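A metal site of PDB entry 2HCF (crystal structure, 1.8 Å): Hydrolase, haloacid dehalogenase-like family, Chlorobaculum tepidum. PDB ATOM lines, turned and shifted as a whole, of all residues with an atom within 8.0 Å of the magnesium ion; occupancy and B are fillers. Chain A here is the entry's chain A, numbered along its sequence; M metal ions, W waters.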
ATOM      1  N   PHE A   9      27.504   1.665  15.683  1.00  0.00           N
ATOM      2  CA  PHE A   9      26.205   2.164  16.120  1.00  0.00           C
ATOM      3  C   PHE A   9      26.372   3.435  16.948  1.00  0.00           C
ATOM      4  O   PHE A   9      27.200   3.486  17.906  1.00  0.00           O
ATOM      5  CB  PHE A   9      25.536   1.157  17.047  1.00  0.00           C
ATOM      6  CG  PHE A   9      24.801   0.034  16.353  1.00  0.00           C
ATOM      7  CD1 PHE A   9      23.458   0.185  15.998  1.00  0.00           C
ATOM      8  CD2 PHE A   9      25.399  -1.216  16.148  1.00  0.00           C
ATOM      9  CE1 PHE A   9      22.772  -0.848  15.385  1.00  0.00           C
ATOM     10  CE2 PHE A   9      24.716  -2.242  15.542  1.00  0.00           C
ATOM     11  CZ  PHE A   9      23.393  -2.055  15.154  1.00  0.00           C
ATOM     12  N   ASP A  10      25.576   4.425  16.583  1.00  0.00           N
ATOM     13  CA  ASP A  10      25.204   5.558  17.439  1.00  0.00           C
ATOM     14  C   ASP A  10      24.323   5.087  18.610  1.00  0.00           C
ATOM     15  O   ASP A  10      23.717   4.054  18.505  1.00  0.00           O
ATOM     16  CB  ASP A  10      24.429   6.536  16.576  1.00  0.00           C
ATOM     17  CG  ASP A  10      23.991   7.774  17.335  1.00  0.00           C
ATOM     18  OD1 ASP A  10      24.899   8.479  17.820  1.00  0.00           O
ATOM     19  OD2 ASP A  10      22.754   8.028  17.419  1.00  0.00           O
ATOM     20  N   ILE A  11      24.294   5.830  19.728  1.00  0.00           N
ATOM     21  CA  ILE A  11      23.474   5.496  20.891  1.00  0.00           C
ATOM     22  C   ILE A  11      22.105   6.236  20.871  1.00  0.00           C
ATOM     23  O   ILE A  11      21.058   5.606  20.586  1.00  0.00           O
ATOM     24  CB  ILE A  11      24.249   5.759  22.189  1.00  0.00           C
ATOM     25  CG1 ILE A  11      25.581   4.968  22.173  1.00  0.00           C
ATOM     26  CG2 ILE A  11      23.408   5.416  23.418  1.00  0.00           C
ATOM     27  CD1 ILE A  11      26.398   5.090  23.431  1.00  0.00           C
ATOM     28  N   ASP A  12      22.108   7.546  21.115  1.00  0.00           N
ATOM     29  CA  ASP A  12      20.862   8.284  21.365  1.00  0.00           C
ATOM     30  C   ASP A  12      20.048   8.457  20.097  1.00  0.00           C
ATOM     31  O   ASP A  12      20.594   8.874  19.049  1.00  0.00           O
ATOM     32  CB  ASP A  12      21.135   9.652  21.994  1.00  0.00           C
ATOM     33  CG  ASP A  12      21.870   9.519  23.357  1.00  0.00           C
ATOM     34  OD1 ASP A  12      23.069   9.239  23.333  1.00  0.00           O
ATOM     35  OD2 ASP A  12      21.235   9.654  24.412  1.00  0.00           O
ATOM     36  N   GLY A  13      18.785   8.046  20.189  1.00  0.00           N
ATOM     37  CA  GLY A  13      17.857   8.063  19.033  1.00  0.00           C
ATOM     38  C   GLY A  13      18.048   6.936  18.016  1.00  0.00           C
ATOM     39  O   GLY A  13      17.384   6.954  16.964  1.00  0.00           O
ATOM     40  N   THR A  14      18.951   5.997  18.314  1.00  0.00           N
ATOM     41  CA  THR A  14      19.273   4.831  17.499  1.00  0.00           C
ATOM     42  C   THR A  14      19.101   3.542  18.300  1.00  0.00           C
ATOM     43  O   THR A  14      18.340   2.650  17.915  1.00  0.00           O
ATOM     44  CB  THR A  14      20.710   4.919  16.976  1.00  0.00           C
ATOM     45  OG1 THR A  14      20.878   6.122  16.196  1.00  0.00           O
ATOM     46  CG2 THR A  14      21.053   3.727  16.105  1.00  0.00           C
ATOM     47  N   LEU A  15      19.817   3.442  19.412  1.00  0.00           N
ATOM     48  CA  LEU A  15      19.623   2.281  20.325  1.00  0.00           C
ATOM     49  C   LEU A  15      18.648   2.564  21.444  1.00  0.00           C
ATOM     50  O   LEU A  15      17.926   1.680  21.902  1.00  0.00           O
ATOM     51  CB  LEU A  15      20.949   1.864  20.917  1.00  0.00           C
ATOM     52  CG  LEU A  15      22.068   1.486  19.933  1.00  0.00           C
ATOM     53  CD1 LEU A  15      23.376   1.240  20.711  1.00  0.00           C
ATOM     54  CD2 LEU A  15      21.659   0.240  19.166  1.00  0.00           C
ATOM     55  N   LEU A  16      18.675   3.783  21.943  1.00  0.00           N
ATOM     56  CA  LEU A  16      17.868   4.140  23.104  1.00  0.00           C
ATOM     57  C   LEU A  16      17.648   5.634  23.139  1.00  0.00           C
ATOM     58  O   LEU A  16      18.244   6.377  22.324  1.00  0.00           O
ATOM     59  CB  LEU A  16      18.550   3.653  24.393  1.00  0.00           C
ATOM     60  CG  LEU A  16      19.997   4.153  24.680  1.00  0.00           C
ATOM     61  CD1 LEU A  16      20.052   5.565  25.275  1.00  0.00           C
ATOM     62  CD2 LEU A  16      20.660   3.169  25.685  1.00  0.00           C
ATOM     63  N   PHE A  45      20.580  19.244  20.011  1.00  0.00           N
ATOM     64  CA  PHE A  45      21.929  18.718  20.042  1.00  0.00           C
ATOM     65  C   PHE A  45      21.986  17.249  19.567  1.00  0.00           C
ATOM     66  O   PHE A  45      22.994  16.577  19.737  1.00  0.00           O
ATOM     67  CB  PHE A  45      22.546  18.968  21.415  1.00  0.00           C
ATOM     68  CG  PHE A  45      22.721  20.465  21.725  1.00  0.00           C
ATOM     69  CD1 PHE A  45      23.484  21.284  20.887  1.00  0.00           C
ATOM     70  CD2 PHE A  45      22.113  21.047  22.834  1.00  0.00           C
ATOM     71  CE1 PHE A  45      23.646  22.633  21.169  1.00  0.00           C
ATOM     72  CE2 PHE A  45      22.277  22.403  23.107  1.00  0.00           C
ATOM     73  CZ  PHE A  45      23.042  23.191  22.257  1.00  0.00           C
ATOM     74  N   SER A  46      20.910  16.812  18.912  1.00  0.00           N
ATOM     75  CA  SER A  46      20.894  15.512  18.220  1.00  0.00           C
ATOM     76  C   SER A  46      22.062  15.333  17.287  1.00  0.00           C
ATOM     77  O   SER A  46      22.282  16.148  16.402  1.00  0.00           O
ATOM     78  CB  SER A  46      19.617  15.367  17.395  1.00  0.00           C
ATOM     79  OG  SER A  46      18.542  15.089  18.241  1.00  0.00           O
ATOM     80  N   GLY A  47      22.818  14.255  17.484  1.00  0.00           N
ATOM     81  CA  GLY A  47      23.929  13.944  16.616  1.00  0.00           C
ATOM     82  C   GLY A  47      25.212  14.709  16.861  1.00  0.00           C
ATOM     83  O   GLY A  47      26.206  14.474  16.199  1.00  0.00           O
ATOM     84  N   LYS A  48      25.206  15.616  17.844  1.00  0.00           N
ATOM     85  CA  LYS A  48      26.372  16.440  18.127  1.00  0.00           C
ATOM     86  C   LYS A  48      27.259  15.823  19.223  1.00  0.00           C
ATOM     87  O   LYS A  48      26.841  14.948  19.982  1.00  0.00           O
ATOM     88  CB  LYS A  48      25.925  17.879  18.435  1.00  0.00           C
ATOM     89  CG  LYS A  48      25.346  18.569  17.187  1.00  0.00           C
ATOM     90  CD  LYS A  48      24.549  19.802  17.533  1.00  0.00           C
ATOM     91  N   LEU A 116      30.013   4.324  17.752  1.00  0.00           N
ATOM     92  CA  LEU A 116      30.496   5.580  17.220  1.00  0.00           C
ATOM     93  C   LEU A 116      29.457   6.617  17.646  1.00  0.00           C
ATOM     94  O   LEU A 116      28.347   6.627  17.069  1.00  0.00           O
ATOM     95  CB  LEU A 116      30.614   5.546  15.688  1.00  0.00           C
ATOM     96  CG  LEU A 116      31.479   6.650  15.097  1.00  0.00           C
ATOM     97  CD1 LEU A 116      31.945   6.294  13.715  1.00  0.00           C
ATOM     98  CD2 LEU A 116      30.765   7.997  15.059  1.00  0.00           C
ATOM     99  N   THR A 117      29.805   7.412  18.675  1.00  0.00           N
ATOM    100  CA  THR A 117      28.817   8.198  19.390  1.00  0.00           C
ATOM    101  C   THR A 117      29.272   9.569  19.838  1.00  0.00           C
ATOM    102  O   THR A 117      30.472   9.804  20.019  1.00  0.00           O
ATOM    103  CB  THR A 117      28.321   7.361  20.591  1.00  0.00           C
ATOM    104  OG1 THR A 117      27.448   8.138  21.400  1.00  0.00           O
ATOM    105  CG2 THR A 117      29.485   6.833  21.387  1.00  0.00           C
ATOM    106  N   GLY A 118      28.314  10.482  20.000  1.00  0.00           N
ATOM    107  CA  GLY A 118      28.577  11.828  20.531  1.00  0.00           C
ATOM    108  C   GLY A 118      28.713  11.838  22.044  1.00  0.00           C
ATOM    109  O   GLY A 118      29.128  12.843  22.631  1.00  0.00           O
ATOM    110  N   ASN A 119      28.341  10.740  22.698  1.00  0.00           N
ATOM    111  CA  ASN A 119      28.562  10.623  24.139  1.00  0.00           C
ATOM    112  C   ASN A 119      30.056  10.488  24.498  1.00  0.00           C
ATOM    113  O   ASN A 119      30.824   9.840  23.785  1.00  0.00           O
ATOM    114  CB  ASN A 119      27.841   9.371  24.691  1.00  0.00           C
ATOM    115  CG  ASN A 119      26.323   9.491  24.704  1.00  0.00           C
ATOM    116  OD1 ASN A 119      25.759  10.060  25.655  1.00  0.00           O
ATOM    117  ND2 ASN A 119      25.645   8.883  23.707  1.00  0.00           N
ATOM    118  N   ARG A 149      32.522  15.174  14.783  1.00  0.00           N
ATOM    119  CA  ARG A 149      32.046  13.776  14.595  1.00  0.00           C
ATOM    120  C   ARG A 149      32.777  13.123  13.429  1.00  0.00           C
ATOM    121  O   ARG A 149      32.968  11.924  13.378  1.00  0.00           O
ATOM    122  CB  ARG A 149      30.522  13.687  14.349  1.00  0.00           C
ATOM    123  CG  ARG A 149      29.972  12.268  14.607  1.00  0.00           C
ATOM    124  CD  ARG A 149      28.517  12.072  14.238  1.00  0.00           C
ATOM    125  NE  ARG A 149      28.149  10.754  14.705  1.00  0.00           N
ATOM    126  CZ  ARG A 149      27.494  10.531  15.820  1.00  0.00           C
ATOM    127  NH1 ARG A 149      27.053  11.546  16.555  1.00  0.00           N
ATOM    128  NH2 ARG A 149      27.237   9.283  16.197  1.00  0.00           N
ATOM    129  N   ILE A 176      25.708   3.293  11.547  1.00  0.00           N
ATOM    130  CA  ILE A 176      24.268   3.364  11.808  1.00  0.00           C
ATOM    131  C   ILE A 176      23.932   4.499  12.790  1.00  0.00           C
ATOM    132  O   ILE A 176      24.501   4.575  13.909  1.00  0.00           O
ATOM    133  CB  ILE A 176      23.748   2.018  12.364  1.00  0.00           C
ATOM    134  CG1 ILE A 176      24.015   0.900  11.356  1.00  0.00           C
ATOM    135  CG2 ILE A 176      22.253   2.105  12.705  1.00  0.00           C
ATOM    136  CD1 ILE A 176      24.000  -0.507  11.952  1.00  0.00           C
ATOM    137  N   GLY A 177      22.961   5.323  12.399  1.00  0.00           N
ATOM    138  CA  GLY A 177      22.422   6.384  13.242  1.00  0.00           C
ATOM    139  C   GLY A 177      21.141   7.051  12.754  1.00  0.00           C
ATOM    140  O   GLY A 177      20.587   6.657  11.746  1.00  0.00           O
ATOM    141  N   ASP A 178      20.730   8.099  13.470  1.00  0.00           N
ATOM    142  CA  ASP A 178      19.408   8.731  13.322  1.00  0.00           C
ATOM    143  C   ASP A 178      19.385  10.174  12.838  1.00  0.00           C
ATOM    144  O   ASP A 178      18.295  10.764  12.793  1.00  0.00           O
ATOM    145  CB  ASP A 178      18.663   8.636  14.652  1.00  0.00           C
ATOM    146  CG  ASP A 178      19.278   9.553  15.740  1.00  0.00           C
ATOM    147  OD1 ASP A 178      20.473   9.329  16.046  1.00  0.00           O
ATOM    148  OD2 ASP A 178      18.558  10.458  16.280  1.00  0.00           O
ATOM    149  N   THR A 179      20.552  10.749  12.481  1.00  0.00           N
ATOM    150  CA  THR A 179      20.635  12.159  12.044  1.00  0.00           C
ATOM    151  C   THR A 179      21.515  12.346  10.840  1.00  0.00           C
ATOM    152  O   THR A 179      22.261  11.446  10.426  1.00  0.00           O
ATOM    153  CB  THR A 179      21.207  13.104  13.146  1.00  0.00           C
ATOM    154  OG1 THR A 179      22.654  13.069  13.109  1.00  0.00           O
ATOM    155  CG2 THR A 179      20.695  12.697  14.532  1.00  0.00           C
ATOM    156  N   HIS A 181      24.149  13.873  10.852  1.00  0.00           N
ATOM    157  CA  HIS A 181      25.543  13.819  11.281  1.00  0.00           C
ATOM    158  C   HIS A 181      26.096  12.401  11.192  1.00  0.00           C
ATOM    159  O   HIS A 181      27.268  12.201  10.865  1.00  0.00           O
ATOM    160  CB  HIS A 181      25.670  14.383  12.690  1.00  0.00           C
ATOM    161  CG  HIS A 181      25.093  15.753  12.827  1.00  0.00           C
ATOM    162  ND1 HIS A 181      25.498  16.805  12.025  1.00  0.00           N
ATOM    163  CD2 HIS A 181      24.111  16.227  13.618  1.00  0.00           C
ATOM    164  CE1 HIS A 181      24.813  17.887  12.364  1.00  0.00           C
ATOM    165  NE2 HIS A 181      23.971  17.569  13.327  1.00  0.00           N
ATOM    166  N   ASP A 182      25.249  11.425  11.487  1.00  0.00           N
ATOM    167  CA  ASP A 182      25.579  10.040  11.301  1.00  0.00           C
ATOM    168  C   ASP A 182      25.843   9.748   9.825  1.00  0.00           C
ATOM    169  O   ASP A 182      26.871   9.171   9.453  1.00  0.00           O
ATOM    170  CB  ASP A 182      24.458   9.168  11.845  1.00  0.00           C
ATOM    171  CG  ASP A 182      24.195   9.465  13.299  1.00  0.00           C
ATOM    172  OD1 ASP A 182      24.967   8.980  14.127  1.00  0.00           O
ATOM    173  OD2 ASP A 182      23.249  10.221  13.623  1.00  0.00           O
ATOM    174  N   VAL A 196      18.203   5.471  10.554  1.00  0.00           N
ATOM    175  CA  VAL A 196      16.961   5.007  11.140  1.00  0.00           C
ATOM    176  C   VAL A 196      16.215   6.211  11.706  1.00  0.00           C
ATOM    177  O   VAL A 196      16.793   7.041  12.420  1.00  0.00           O
ATOM    178  CB  VAL A 196      17.252   3.884  12.193  1.00  0.00           C
ATOM    179  CG1 VAL A 196      18.152   4.386  13.279  1.00  0.00           C
ATOM    180  CG2 VAL A 196      15.965   3.304  12.728  1.00  0.00           C
ATOM    181  N   THR A 198      14.199   7.014  13.978  1.00  0.00           N
ATOM    182  CA  THR A 198      13.699   6.861  15.349  1.00  0.00           C
ATOM    183  C   THR A 198      14.162   7.990  16.279  1.00  0.00           C
ATOM    184  O   THR A 198      13.956   7.935  17.489  1.00  0.00           O
ATOM    185  CB  THR A 198      14.112   5.494  15.946  1.00  0.00           C
ATOM    186  OG1 THR A 198      15.487   5.235  15.691  1.00  0.00           O
ATOM    187  CG2 THR A 198      13.304   4.394  15.346  1.00  0.00           C
ATOM    188  N   GLY A 199      14.744   9.051  15.715  1.00  0.00           N
ATOM    189  CA  GLY A 199      15.080  10.224  16.499  1.00  0.00           C
ATOM    190  C   GLY A 199      14.145  11.347  16.173  1.00  0.00           C
ATOM    191  O   GLY A 199      12.928  11.131  15.912  1.00  0.00           O
ATOM    192  N   ASN A 200      14.690  12.544  16.111  1.00  0.00           N
ATOM    193  CA  ASN A 200      13.888  13.719  15.865  1.00  0.00           C
ATOM    194  C   ASN A 200      13.724  14.074  14.380  1.00  0.00           C
ATOM    195  O   ASN A 200      13.124  15.088  14.073  1.00  0.00           O
ATOM    196  CB  ASN A 200      14.424  14.897  16.680  1.00  0.00           C
ATOM    197  CG  ASN A 200      14.371  14.619  18.171  1.00  0.00           C
ATOM    198  OD1 ASN A 200      13.476  13.927  18.643  1.00  0.00           O
ATOM    199  ND2 ASN A 200      15.349  15.106  18.898  1.00  0.00           N
ATOM    200  N   PHE A 201      14.194  13.211  13.474  1.00  0.00           N
ATOM    201  CA  PHE A 201      14.178  13.534  12.019  1.00  0.00           C
ATOM    202  C   PHE A 201      13.431  12.446  11.272  1.00  0.00           C
ATOM    203  O   PHE A 201      13.657  11.265  11.488  1.00  0.00           O
ATOM    204  CB  PHE A 201      15.587  13.709  11.469  1.00  0.00           C
ATOM    205  CG  PHE A 201      16.375  14.680  12.272  1.00  0.00           C
ATOM    206  CD1 PHE A 201      16.235  16.051  12.057  1.00  0.00           C
ATOM    207  CD2 PHE A 201      17.164  14.228  13.339  1.00  0.00           C
ATOM    208  CE1 PHE A 201      16.900  16.955  12.874  1.00  0.00           C
ATOM    209  CE2 PHE A 201      17.835  15.121  14.135  1.00  0.00           C
ATOM    210  CZ  PHE A 201      17.701  16.476  13.921  1.00  0.00           C
HETATM  211 MG    MG M   1      21.815   9.830  17.583  1.00  0.00          MG
HETATM  212  O   HOH W   1      23.134  10.619  19.047  1.00  0.00           O
HETATM  213  O   HOH W   2      23.200  10.621  16.264  1.00  0.00           O
HETATM  214  O   HOH W   3      20.405  11.536  17.938  1.00  0.00           O
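N of Asp 178 sits at hydrogen-bond distance from OD2 of Asp 182, at 3.3 Å. The side-chain carboxylate of Asp 10 lies close to the side-chain hydroxyl of Thr 14, 2.9 Å away. OG1 of Thr 14 sits at hydrogen-bond distance from N of Asp 178, at 3.4 Å. OD1 of Asp 12 is in hydrogen-bond range of ND2 of Asn 119 (2.6 Å). The backbone NH of Asp 10 sits at hydrogen-bond distance from the backbone carbonyl oxygen of Ile 176 (2.9 Å). The side-chain carboxylate (OD1) of Asp 10 lies within salt-bridge range of the guanidinium group (NH2) of Arg 149, at 3.0 Å.
Of the 28 residues printed, 3 come within 4 Å of the magnesium ion.
The magnesium ion is bound by OD2 of Asp 10 (2.0 Å), water W2 (2.1 Å), OD1 of Asp 178 (2.1 Å), water W1 (2.1 Å), O of Asp 12 (2.1 Å) and water W3 (2.2 Å).
Water W2 lies within hydrogen-bond range of OD2 of Asp 182 (2.7 Å) and OD1 of Asp 10 (3.1 Å).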
